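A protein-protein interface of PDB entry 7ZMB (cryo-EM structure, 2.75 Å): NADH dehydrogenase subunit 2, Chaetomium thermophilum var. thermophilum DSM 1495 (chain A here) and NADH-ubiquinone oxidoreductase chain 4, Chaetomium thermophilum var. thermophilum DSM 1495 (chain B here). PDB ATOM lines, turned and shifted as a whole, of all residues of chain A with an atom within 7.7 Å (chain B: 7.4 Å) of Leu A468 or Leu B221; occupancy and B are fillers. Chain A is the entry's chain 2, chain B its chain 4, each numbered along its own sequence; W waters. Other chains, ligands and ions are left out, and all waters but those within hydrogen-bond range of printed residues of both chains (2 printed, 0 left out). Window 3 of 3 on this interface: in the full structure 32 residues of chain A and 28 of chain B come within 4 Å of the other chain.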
ATOM      1  N   LEU A 323      29.403  14.747 -30.376  1.00  0.00           N
ATOM      2  CA  LEU A 323      28.025  14.534 -29.956  1.00  0.00           C
ATOM      3  C   LEU A 323      27.674  15.394 -28.745  1.00  0.00           C
ATOM      4  O   LEU A 323      26.704  16.155 -28.784  1.00  0.00           O
ATOM      5  CB  LEU A 323      27.789  13.049 -29.683  1.00  0.00           C
ATOM      6  CG  LEU A 323      27.858  12.176 -30.945  1.00  0.00           C
ATOM      7  CD1 LEU A 323      27.812  10.695 -30.626  1.00  0.00           C
ATOM      8  CD2 LEU A 323      26.777  12.542 -31.947  1.00  0.00           C
ATOM      9  N   LEU A 353      31.458   8.468 -36.117  1.00  0.00           N
ATOM     10  CA  LEU A 353      31.185   7.164 -35.524  1.00  0.00           C
ATOM     11  C   LEU A 353      31.043   6.086 -36.589  1.00  0.00           C
ATOM     12  O   LEU A 353      31.532   4.966 -36.411  1.00  0.00           O
ATOM     13  CB  LEU A 353      29.923   7.236 -34.666  1.00  0.00           C
ATOM     14  CG  LEU A 353      29.417   5.917 -34.087  1.00  0.00           C
ATOM     15  CD1 LEU A 353      30.404   5.338 -33.109  1.00  0.00           C
ATOM     16  CD2 LEU A 353      28.063   6.099 -33.458  1.00  0.00           C
ATOM     17  N   GLN A 452      19.446   5.802 -38.122  1.00  0.00           N
ATOM     18  CA  GLN A 452      19.166   4.380 -37.802  1.00  0.00           C
ATOM     19  C   GLN A 452      20.232   3.471 -38.426  1.00  0.00           C
ATOM     20  O   GLN A 452      20.627   2.505 -37.764  1.00  0.00           O
ATOM     21  CB  GLN A 452      17.735   4.061 -38.237  1.00  0.00           C
ATOM     22  CG  GLN A 452      17.370   2.585 -38.221  1.00  0.00           C
ATOM     23  CD  GLN A 452      17.566   1.935 -39.568  1.00  0.00           C
ATOM     24  OE1 GLN A 452      17.538   2.591 -40.605  1.00  0.00           O
ATOM     25  NE2 GLN A 452      17.776   0.630 -39.560  1.00  0.00           N
ATOM     26  N   LEU A 455      23.305   3.688 -36.325  1.00  0.00           N
ATOM     27  CA  LEU A 455      23.081   3.004 -35.056  1.00  0.00           C
ATOM     28  C   LEU A 455      23.077   1.493 -35.228  1.00  0.00           C
ATOM     29  O   LEU A 455      23.597   0.770 -34.376  1.00  0.00           O
ATOM     30  CB  LEU A 455      21.768   3.472 -34.435  1.00  0.00           C
ATOM     31  CG  LEU A 455      21.712   4.907 -33.926  1.00  0.00           C
ATOM     32  CD1 LEU A 455      20.289   5.259 -33.543  1.00  0.00           C
ATOM     33  CD2 LEU A 455      22.660   5.120 -32.760  1.00  0.00           C
ATOM     34  N   SER A 456      22.489   1.001 -36.298  1.00  0.00           N
ATOM     35  CA  SER A 456      22.437  -0.460 -36.562  1.00  0.00           C
ATOM     36  C   SER A 456      23.850  -1.009 -36.730  1.00  0.00           C
ATOM     37  O   SER A 456      24.126  -2.090 -36.196  1.00  0.00           O
ATOM     38  CB  SER A 456      21.599  -0.747 -37.775  1.00  0.00           C
ATOM     39  OG  SER A 456      20.348  -1.308 -37.415  1.00  0.00           O
ATOM     40  N   LEU A 459      25.751  -0.898 -33.308  1.00  0.00           N
ATOM     41  CA  LEU A 459      25.209  -1.923 -32.386  1.00  0.00           C
ATOM     42  C   LEU A 459      25.742  -3.293 -32.794  1.00  0.00           C
ATOM     43  O   LEU A 459      26.098  -4.072 -31.902  1.00  0.00           O
ATOM     44  CB  LEU A 459      23.678  -1.894 -32.415  1.00  0.00           C
ATOM     45  CG  LEU A 459      23.019  -0.880 -31.484  1.00  0.00           C
ATOM     46  CD1 LEU A 459      21.525  -0.816 -31.745  1.00  0.00           C
ATOM     47  CD2 LEU A 459      23.292  -1.223 -30.031  1.00  0.00           C
ATOM     48  N   TYR A 463      29.895  -1.404 -30.492  1.00  0.00           N
ATOM     49  CA  TYR A 463      30.023  -0.005 -30.019  1.00  0.00           C
ATOM     50  C   TYR A 463      28.699   0.345 -29.345  1.00  0.00           C
ATOM     51  O   TYR A 463      28.007   1.266 -29.801  1.00  0.00           O
ATOM     52  CB  TYR A 463      30.388   0.903 -31.195  1.00  0.00           C
ATOM     53  CG  TYR A 463      31.720   0.628 -31.845  1.00  0.00           C
ATOM     54  CD1 TYR A 463      31.893  -0.445 -32.700  1.00  0.00           C
ATOM     55  CD2 TYR A 463      32.802   1.461 -31.625  1.00  0.00           C
ATOM     56  CE1 TYR A 463      33.113  -0.699 -33.304  1.00  0.00           C
ATOM     57  CE2 TYR A 463      34.026   1.227 -32.227  1.00  0.00           C
ATOM     58  CZ  TYR A 463      34.183   0.142 -33.071  1.00  0.00           C
ATOM     59  OH  TYR A 463      35.386  -0.095 -33.666  1.00  0.00           O
ATOM     60  N   ILE A 464      28.376  -0.364 -28.268  1.00  0.00           N
ATOM     61  CA  ILE A 464      27.064  -0.181 -27.592  1.00  0.00           C
ATOM     62  C   ILE A 464      27.130   1.121 -26.804  1.00  0.00           C
ATOM     63  O   ILE A 464      26.096   1.795 -26.698  1.00  0.00           O
ATOM     64  CB  ILE A 464      26.760  -1.386 -26.680  1.00  0.00           C
ATOM     65  CG1 ILE A 464      27.149  -2.713 -27.336  1.00  0.00           C
ATOM     66  CG2 ILE A 464      25.307  -1.383 -26.229  1.00  0.00           C
ATOM     67  CD1 ILE A 464      26.368  -3.035 -28.589  1.00  0.00           C
ATOM     68  N   PHE A 465      28.312   1.456 -26.289  1.00  0.00           N
ATOM     69  CA  PHE A 465      28.387   2.649 -25.458  1.00  0.00           C
ATOM     70  C   PHE A 465      28.222   3.919 -26.287  1.00  0.00           C
ATOM     71  O   PHE A 465      27.514   4.843 -25.875  1.00  0.00           O
ATOM     72  CB  PHE A 465      29.708   2.657 -24.687  1.00  0.00           C
ATOM     73  CG  PHE A 465      29.861   3.816 -23.760  1.00  0.00           C
ATOM     74  CD1 PHE A 465      29.334   3.766 -22.487  1.00  0.00           C
ATOM     75  CD2 PHE A 465      30.537   4.957 -24.157  1.00  0.00           C
ATOM     76  CE1 PHE A 465      29.470   4.831 -21.627  1.00  0.00           C
ATOM     77  CE2 PHE A 465      30.673   6.025 -23.302  1.00  0.00           C
ATOM     78  CZ  PHE A 465      30.139   5.961 -22.034  1.00  0.00           C
ATOM     79  N   LEU A 466      28.873   3.986 -27.451  1.00  0.00           N
ATOM     80  CA  LEU A 466      28.705   5.136 -28.337  1.00  0.00           C
ATOM     81  C   LEU A 466      27.292   5.238 -28.885  1.00  0.00           C
ATOM     82  O   LEU A 466      26.821   6.343 -29.167  1.00  0.00           O
ATOM     83  CB  LEU A 466      29.701   5.081 -29.497  1.00  0.00           C
ATOM     84  CG  LEU A 466      31.125   5.605 -29.294  1.00  0.00           C
ATOM     85  CD1 LEU A 466      31.080   7.082 -29.018  1.00  0.00           C
ATOM     86  CD2 LEU A 466      31.826   4.886 -28.164  1.00  0.00           C
ATOM     87  N   SER A 467      26.614   4.106 -29.077  1.00  0.00           N
ATOM     88  CA  SER A 467      25.216   4.153 -29.484  1.00  0.00           C
ATOM     89  C   SER A 467      24.358   4.802 -28.410  1.00  0.00           C
ATOM     90  O   SER A 467      23.432   5.557 -28.718  1.00  0.00           O
ATOM     91  CB  SER A 467      24.709   2.750 -29.794  1.00  0.00           C
ATOM     92  OG  SER A 467      25.161   2.315 -31.056  1.00  0.00           O
ATOM     93  N   LEU A 468      24.643   4.506 -27.142  1.00  0.00           N
ATOM     94  CA  LEU A 468      23.875   5.087 -26.051  1.00  0.00           C
ATOM     95  C   LEU A 468      24.157   6.577 -25.903  1.00  0.00           C
ATOM     96  O   LEU A 468      23.240   7.361 -25.639  1.00  0.00           O
ATOM     97  CB  LEU A 468      24.174   4.347 -24.756  1.00  0.00           C
ATOM     98  CG  LEU A 468      23.634   2.920 -24.699  1.00  0.00           C
ATOM     99  CD1 LEU A 468      24.166   2.201 -23.472  1.00  0.00           C
ATOM    100  CD2 LEU A 468      22.125   2.919 -24.729  1.00  0.00           C
ATOM    101  N   ILE A 469      25.414   6.987 -26.069  1.00  0.00           N
ATOM    102  CA  ILE A 469      25.734   8.411 -26.090  1.00  0.00           C
ATOM    103  C   ILE A 469      24.921   9.110 -27.166  1.00  0.00           C
ATOM    104  O   ILE A 469      24.291  10.143 -26.921  1.00  0.00           O
ATOM    105  CB  ILE A 469      27.244   8.630 -26.312  1.00  0.00           C
ATOM    106  CG1 ILE A 469      28.076   7.995 -25.199  1.00  0.00           C
ATOM    107  CG2 ILE A 469      27.552  10.108 -26.442  1.00  0.00           C
ATOM    108  CD1 ILE A 469      27.855   8.602 -23.854  1.00  0.00           C
ATOM    109  N   ALA A 470      24.898   8.532 -28.367  1.00  0.00           N
ATOM    110  CA  ALA A 470      24.280   9.193 -29.510  1.00  0.00           C
ATOM    111  C   ALA A 470      22.781   9.372 -29.320  1.00  0.00           C
ATOM    112  O   ALA A 470      22.224  10.405 -29.706  1.00  0.00           O
ATOM    113  CB  ALA A 470      24.573   8.407 -30.784  1.00  0.00           C
ATOM    114  N   ILE A 471      22.098   8.375 -28.749  1.00  0.00           N
ATOM    115  CA  ILE A 471      20.653   8.502 -28.591  1.00  0.00           C
ATOM    116  C   ILE A 471      20.314   9.530 -27.518  1.00  0.00           C
ATOM    117  O   ILE A 471      19.374  10.316 -27.674  1.00  0.00           O
ATOM    118  CB  ILE A 471      19.992   7.136 -28.321  1.00  0.00           C
ATOM    119  CG1 ILE A 471      20.387   6.552 -26.963  1.00  0.00           C
ATOM    120  CG2 ILE A 471      20.290   6.168 -29.449  1.00  0.00           C
ATOM    121  CD1 ILE A 471      19.499   5.407 -26.517  1.00  0.00           C
ATOM    122  N   ILE A 472      21.071   9.550 -26.419  1.00  0.00           N
ATOM    123  CA  ILE A 472      20.842  10.548 -25.383  1.00  0.00           C
ATOM    124  C   ILE A 472      21.210  11.928 -25.897  1.00  0.00           C
ATOM    125  O   ILE A 472      20.547  12.924 -25.592  1.00  0.00           O
ATOM    126  CB  ILE A 472      21.625  10.182 -24.109  1.00  0.00           C
ATOM    127  CG1 ILE A 472      21.189   8.814 -23.605  1.00  0.00           C
ATOM    128  CG2 ILE A 472      21.463  11.243 -23.029  1.00  0.00           C
ATOM    129  CD1 ILE A 472      19.738   8.742 -23.240  1.00  0.00           C
ATOM    130  N   THR A 473      22.270  12.001 -26.691  1.00  0.00           N
ATOM    131  CA  THR A 473      22.688  13.257 -27.293  1.00  0.00           C
ATOM    132  C   THR A 473      21.612  13.833 -28.206  1.00  0.00           C
ATOM    133  O   THR A 473      21.390  15.047 -28.225  1.00  0.00           O
ATOM    134  CB  THR A 473      23.988  13.025 -28.051  1.00  0.00           C
ATOM    135  OG1 THR A 473      24.995  12.578 -27.139  1.00  0.00           O
ATOM    136  CG2 THR A 473      24.428  14.239 -28.724  1.00  0.00           C
ATOM    137  N   SER A 474      20.933  12.975 -28.964  1.00  0.00           N
ATOM    138  CA  SER A 474      19.954  13.453 -29.929  1.00  0.00           C
ATOM    139  C   SER A 474      18.763  14.122 -29.251  1.00  0.00           C
ATOM    140  O   SER A 474      18.259  15.139 -29.739  1.00  0.00           O
ATOM    141  CB  SER A 474      19.496  12.301 -30.815  1.00  0.00           C
ATOM    142  OG  SER A 474      20.546  11.891 -31.664  1.00  0.00           O
ATOM    143  N   TYR B 179       7.725   0.921 -35.650  1.00  0.00           N
ATOM    144  CA  TYR B 179       8.429   2.063 -35.090  1.00  0.00           C
ATOM    145  C   TYR B 179       8.373   3.276 -36.013  1.00  0.00           C
ATOM    146  O   TYR B 179       8.342   4.412 -35.540  1.00  0.00           O
ATOM    147  CB  TYR B 179       9.877   1.672 -34.806  1.00  0.00           C
ATOM    148  CG  TYR B 179      10.707   2.770 -34.200  1.00  0.00           C
ATOM    149  CD1 TYR B 179      11.391   3.666 -34.995  1.00  0.00           C
ATOM    150  CD2 TYR B 179      10.803   2.909 -32.830  1.00  0.00           C
ATOM    151  CE1 TYR B 179      12.138   4.672 -34.440  1.00  0.00           C
ATOM    152  CE2 TYR B 179      11.552   3.904 -32.274  1.00  0.00           C
ATOM    153  CZ  TYR B 179      12.218   4.782 -33.081  1.00  0.00           C
ATOM    154  OH  TYR B 179      12.970   5.782 -32.527  1.00  0.00           O
ATOM    155  N   GLY B 215      12.122   7.490 -25.141  1.00  0.00           N
ATOM    156  CA  GLY B 215      11.713   6.100 -24.874  1.00  0.00           C
ATOM    157  C   GLY B 215      11.817   5.287 -26.138  1.00  0.00           C
ATOM    158  O   GLY B 215      12.293   4.154 -26.067  1.00  0.00           O
ATOM    159  N   SER B 216      11.429   5.900 -27.254  1.00  0.00           N
ATOM    160  CA  SER B 216      11.443   5.207 -28.560  1.00  0.00           C
ATOM    161  C   SER B 216      12.871   4.863 -28.960  1.00  0.00           C
ATOM    162  O   SER B 216      13.050   3.832 -29.588  1.00  0.00           O
ATOM    163  CB  SER B 216      10.803   6.075 -29.593  1.00  0.00           C
ATOM    164  OG  SER B 216      11.739   6.993 -30.134  1.00  0.00           O
ATOM    165  N   LEU B 217      13.838   5.717 -28.630  1.00  0.00           N
ATOM    166  CA  LEU B 217      15.242   5.475 -29.036  1.00  0.00           C
ATOM    167  C   LEU B 217      15.723   4.243 -28.284  1.00  0.00           C
ATOM    168  O   LEU B 217      16.470   3.453 -28.878  1.00  0.00           O
ATOM    169  CB  LEU B 217      16.091   6.728 -28.833  1.00  0.00           C
ATOM    170  CG  LEU B 217      15.805   7.852 -29.825  1.00  0.00           C
ATOM    171  CD1 LEU B 217      16.626   9.090 -29.510  1.00  0.00           C
ATOM    172  CD2 LEU B 217      16.052   7.393 -31.252  1.00  0.00           C
ATOM    173  N   PHE B 218      15.288   4.066 -27.036  1.00  0.00           N
ATOM    174  CA  PHE B 218      15.618   2.819 -26.357  1.00  0.00           C
ATOM    175  C   PHE B 218      14.898   1.640 -26.998  1.00  0.00           C
ATOM    176  O   PHE B 218      15.464   0.545 -27.101  1.00  0.00           O
ATOM    177  CB  PHE B 218      15.308   2.934 -24.871  1.00  0.00           C
ATOM    178  CG  PHE B 218      16.300   3.771 -24.134  1.00  0.00           C
ATOM    179  CD1 PHE B 218      17.441   3.203 -23.599  1.00  0.00           C
ATOM    180  CD2 PHE B 218      16.110   5.131 -24.006  1.00  0.00           C
ATOM    181  CE1 PHE B 218      18.357   3.972 -22.950  1.00  0.00           C
ATOM    182  CE2 PHE B 218      17.017   5.900 -23.358  1.00  0.00           C
ATOM    183  CZ  PHE B 218      18.143   5.325 -22.823  1.00  0.00           C
ATOM    184  N   LEU B 219      13.661   1.846 -27.458  1.00  0.00           N
ATOM    185  CA  LEU B 219      12.981   0.819 -28.238  1.00  0.00           C
ATOM    186  C   LEU B 219      13.693   0.564 -29.553  1.00  0.00           C
ATOM    187  O   LEU B 219      13.820  -0.586 -29.984  1.00  0.00           O
ATOM    188  CB  LEU B 219      11.535   1.227 -28.500  1.00  0.00           C
ATOM    189  CG  LEU B 219      10.633   0.355 -29.371  1.00  0.00           C
ATOM    190  CD1 LEU B 219      10.346  -0.957 -28.705  1.00  0.00           C
ATOM    191  CD2 LEU B 219       9.340   1.065 -29.683  1.00  0.00           C
ATOM    192  N   LEU B 220      14.156   1.629 -30.214  1.00  0.00           N
ATOM    193  CA  LEU B 220      14.784   1.474 -31.521  1.00  0.00           C
ATOM    194  C   LEU B 220      16.060   0.645 -31.431  1.00  0.00           C
ATOM    195  O   LEU B 220      16.342  -0.158 -32.320  1.00  0.00           O
ATOM    196  CB  LEU B 220      15.064   2.843 -32.136  1.00  0.00           C
ATOM    197  CG  LEU B 220      15.732   2.900 -33.515  1.00  0.00           C
ATOM    198  CD1 LEU B 220      14.834   2.363 -34.631  1.00  0.00           C
ATOM    199  CD2 LEU B 220      16.176   4.308 -33.818  1.00  0.00           C
ATOM    200  N   LEU B 221      16.839   0.819 -30.363  1.00  0.00           N
ATOM    201  CA  LEU B 221      18.041   0.009 -30.181  1.00  0.00           C
ATOM    202  C   LEU B 221      17.723  -1.467 -30.021  1.00  0.00           C
ATOM    203  O   LEU B 221      18.579  -2.305 -30.311  1.00  0.00           O
ATOM    204  CB  LEU B 221      18.842   0.482 -28.967  1.00  0.00           C
ATOM    205  CG  LEU B 221      19.466   1.880 -28.971  1.00  0.00           C
ATOM    206  CD1 LEU B 221      20.580   1.958 -27.954  1.00  0.00           C
ATOM    207  CD2 LEU B 221      19.963   2.286 -30.342  1.00  0.00           C
ATOM    208  N   SER B 222      16.515  -1.800 -29.564  1.00  0.00           N
ATOM    209  CA  SER B 222      16.110  -3.190 -29.418  1.00  0.00           C
ATOM    210  C   SER B 222      15.618  -3.764 -30.738  1.00  0.00           C
ATOM    211  O   SER B 222      15.939  -4.902 -31.088  1.00  0.00           O
ATOM    212  CB  SER B 222      15.019  -3.298 -28.357  1.00  0.00           C
ATOM    213  OG  SER B 222      15.370  -2.579 -27.192  1.00  0.00           O
ATOM    214  N   ILE B 223      14.831  -2.982 -31.472  1.00  0.00           N
ATOM    215  CA  ILE B 223      14.338  -3.408 -32.774  1.00  0.00           C
ATOM    216  C   ILE B 223      15.499  -3.617 -33.729  1.00  0.00           C
ATOM    217  O   ILE B 223      15.488  -4.534 -34.558  1.00  0.00           O
ATOM    218  CB  ILE B 223      13.330  -2.373 -33.304  1.00  0.00           C
ATOM    219  CG1 ILE B 223      12.143  -2.268 -32.344  1.00  0.00           C
ATOM    220  CG2 ILE B 223      12.890  -2.704 -34.716  1.00  0.00           C
ATOM    221  CD1 ILE B 223      11.298  -1.043 -32.546  1.00  0.00           C
ATOM    222  N   LEU B 224      16.527  -2.777 -33.615  1.00  0.00           N
ATOM    223  CA  LEU B 224      17.682  -2.893 -34.491  1.00  0.00           C
ATOM    224  C   LEU B 224      18.511  -4.122 -34.153  1.00  0.00           C
ATOM    225  O   LEU B 224      19.047  -4.779 -35.048  1.00  0.00           O
ATOM    226  CB  LEU B 224      18.520  -1.619 -34.413  1.00  0.00           C
ATOM    227  CG  LEU B 224      17.816  -0.410 -35.019  1.00  0.00           C
ATOM    228  CD1 LEU B 224      18.741   0.786 -35.157  1.00  0.00           C
ATOM    229  CD2 LEU B 224      17.197  -0.784 -36.344  1.00  0.00           C
ATOM    230  N   THR B 225      18.624  -4.451 -32.868  1.00  0.00           N
ATOM    231  CA  THR B 225      19.279  -5.692 -32.472  1.00  0.00           C
ATOM    232  C   THR B 225      18.545  -6.912 -33.020  1.00  0.00           C
ATOM    233  O   THR B 225      19.176  -7.850 -33.510  1.00  0.00           O
ATOM    234  CB  THR B 225      19.388  -5.753 -30.951  1.00  0.00           C
ATOM    235  OG1 THR B 225      20.295  -4.742 -30.506  1.00  0.00           O
ATOM    236  CG2 THR B 225      19.883  -7.107 -30.488  1.00  0.00           C
ATOM    237  N   MET B 226      17.211  -6.915 -32.962  1.00  0.00           N
ATOM    238  CA  MET B 226      16.461  -8.045 -33.504  1.00  0.00           C
ATOM    239  C   MET B 226      16.723  -8.223 -34.987  1.00  0.00           C
ATOM    240  O   MET B 226      16.879  -9.350 -35.466  1.00  0.00           O
ATOM    241  CB  MET B 226      14.961  -7.860 -33.287  1.00  0.00           C
ATOM    242  CG  MET B 226      14.527  -7.688 -31.865  1.00  0.00           C
ATOM    243  SD  MET B 226      12.737  -7.703 -31.825  1.00  0.00           S
ATOM    244  CE  MET B 226      12.440  -7.262 -30.133  1.00  0.00           C
ATOM    245  N   SER B 228      19.289  -7.412 -36.761  1.00  0.00           N
ATOM    246  CA  SER B 228      20.627  -7.907 -37.037  1.00  0.00           C
ATOM    247  C   SER B 228      20.782  -9.380 -36.702  1.00  0.00           C
ATOM    248  O   SER B 228      21.674 -10.033 -37.250  1.00  0.00           O
ATOM    249  CB  SER B 228      21.660  -7.091 -36.268  1.00  0.00           C
ATOM    250  OG  SER B 228      21.213  -6.851 -34.954  1.00  0.00           O
ATOM    251  N   PHE B 250      17.937  -8.292 -22.294  1.00  0.00           N
ATOM    252  CA  PHE B 250      18.336  -6.972 -22.759  1.00  0.00           C
ATOM    253  C   PHE B 250      17.409  -6.445 -23.841  1.00  0.00           C
ATOM    254  O   PHE B 250      17.192  -5.236 -23.922  1.00  0.00           O
ATOM    255  CB  PHE B 250      19.782  -6.990 -23.229  1.00  0.00           C
ATOM    256  CG  PHE B 250      20.751  -7.204 -22.120  1.00  0.00           C
ATOM    257  CD1 PHE B 250      20.993  -6.188 -21.211  1.00  0.00           C
ATOM    258  CD2 PHE B 250      21.405  -8.409 -21.967  1.00  0.00           C
ATOM    259  CE1 PHE B 250      21.867  -6.369 -20.184  1.00  0.00           C
ATOM    260  CE2 PHE B 250      22.281  -8.592 -20.937  1.00  0.00           C
ATOM    261  CZ  PHE B 250      22.513  -7.571 -20.043  1.00  0.00           C
ATOM    262  N   LEU B 251      16.836  -7.322 -24.659  1.00  0.00           N
ATOM    263  CA  LEU B 251      15.807  -6.862 -25.579  1.00  0.00           C
ATOM    264  C   LEU B 251      14.556  -6.417 -24.838  1.00  0.00           C
ATOM    265  O   LEU B 251      13.883  -5.483 -25.283  1.00  0.00           O
ATOM    266  CB  LEU B 251      15.470  -7.952 -26.590  1.00  0.00           C
ATOM    267  CG  LEU B 251      16.521  -8.133 -27.675  1.00  0.00           C
ATOM    268  CD1 LEU B 251      16.018  -9.065 -28.738  1.00  0.00           C
ATOM    269  CD2 LEU B 251      16.909  -6.789 -28.259  1.00  0.00           C
ATOM    270  N   PHE B 253      14.334  -4.859 -21.901  1.00  0.00           N
ATOM    271  CA  PHE B 253      14.608  -3.463 -21.628  1.00  0.00           C
ATOM    272  C   PHE B 253      14.885  -2.731 -22.934  1.00  0.00           C
ATOM    273  O   PHE B 253      15.276  -3.321 -23.942  1.00  0.00           O
ATOM    274  CB  PHE B 253      15.780  -3.331 -20.669  1.00  0.00           C
ATOM    275  CG  PHE B 253      15.706  -4.261 -19.507  1.00  0.00           C
ATOM    276  CD1 PHE B 253      14.559  -4.336 -18.740  1.00  0.00           C
ATOM    277  CD2 PHE B 253      16.783  -5.061 -19.174  1.00  0.00           C
ATOM    278  CE1 PHE B 253      14.492  -5.189 -17.662  1.00  0.00           C
ATOM    279  CE2 PHE B 253      16.714  -5.924 -18.099  1.00  0.00           C
ATOM    280  CZ  PHE B 253      15.574  -5.986 -17.344  1.00  0.00           C
ATOM    281  N   GLY B 254      14.660  -1.431 -22.917  1.00  0.00           N
ATOM    282  CA  GLY B 254      14.608  -0.718 -24.170  1.00  0.00           C
ATOM    283  C   GLY B 254      13.191  -0.736 -24.691  1.00  0.00           C
ATOM    284  O   GLY B 254      12.582   0.321 -24.862  1.00  0.00           O
ATOM    285  N   ILE B 255      12.642  -1.927 -24.932  1.00  0.00           N
ATOM    286  CA  ILE B 255      11.229  -2.012 -25.278  1.00  0.00           C
ATOM    287  C   ILE B 255      10.373  -1.633 -24.081  1.00  0.00           C
ATOM    288  O   ILE B 255       9.410  -0.869 -24.206  1.00  0.00           O
ATOM    289  CB  ILE B 255      10.867  -3.412 -25.798  1.00  0.00           C
ATOM    290  CG1 ILE B 255      11.699  -3.770 -27.025  1.00  0.00           C
ATOM    291  CG2 ILE B 255       9.370  -3.480 -26.118  1.00  0.00           C
ATOM    292  CD1 ILE B 255      11.431  -5.146 -27.535  1.00  0.00           C
HETATM  293  O   HOH W   1      19.507  -4.497 -37.544  1.00  0.00           O
HETATM  294  O   HOH W   2      22.046  -3.637 -34.951  1.00  0.00           O
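The backbone carbonyl oxygen (O) of Phe B218 lies within hydrogen-bond range of the side-chain hydroxyl (OG) of Ser B222 (3.1 Å). The backbone carbonyl oxygen of Leu B221 sits at hydrogen-bond distance from the side-chain hydroxyl of Thr B225 (3.0 Å). The backbone carbonyl oxygen of Leu B224 lies within hydrogen-bond range of the side-chain hydroxyl of Ser B228, 3.0 Å away.
Among the printed residues, pairs that only touch across the chains: Ser A456 with Leu B224 (3.4 Å), Ile A471 with Leu B217 (3.5 Å), Gln A452 with Leu B224 (3.6 Å), Leu A459 with Leu B221 (3.6 Å), Leu A468 with Leu B221 (3.7 Å), Ile A472 with Phe B218 (3.8 Å), Ile A471 with Leu B221 (3.9 Å) and Ile A471 with Phe B218 (3.9 Å).
Of the printed residues of chain B, Ser A456 touches Leu B224 (3.4 Å). Of the printed residues of chain B, Leu A459 touches Leu B221 (3.6 Å). Ile A464 touches none of the printed residues of chain B. Of the printed residues of chain B, Ile A472 touches Phe B218. Tyr B179 touches none of the printed residues of chain A. Of the printed residues of chain A, Leu B217 touches Ile A471. Of chain A, only Leu A459 (3.6 Å), Leu A468 (3.7 Å) and Ile A471 (3.9 Å) come within 4 Å of Leu B221. The nearest residue of chain B that does not touch Leu A468 is Phe B218 (4.3 Å). The nearest printed residue of chain A that does not touch Phe B218 is Leu A468 (4.3 Å).
Of the 18 printed residues of chain A, 6 touch a printed residue of chain B. Hydrophobic or aromatic side chains of chain A that line the printed part of chain B: Leu A459, Leu A468, Ile A471 and Ile A472. Along chain A the printed residues that touch a printed residue of chain B span positions 452 to 472. Of the 19 printed residues of chain B, 4 touch a printed residue of chain A. Among the printed residues, no Asp or Glu carboxylate lies within 4 Å of a Lys or Arg side-chain nitrogen of the other chain.
Water W1 lies within hydrogen-bond range of the backbone carbonyl oxygen (O) of Leu B224, the backbone NH (N) of Ser B228 and the side-chain hydroxyl (OG) of Ser A456. Water W2 lies within hydrogen-bond range of O of Ser A456 (2.9 Å), O of Leu B224 (3.2 Å) and OG of Ser B228 (3.3 Å).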
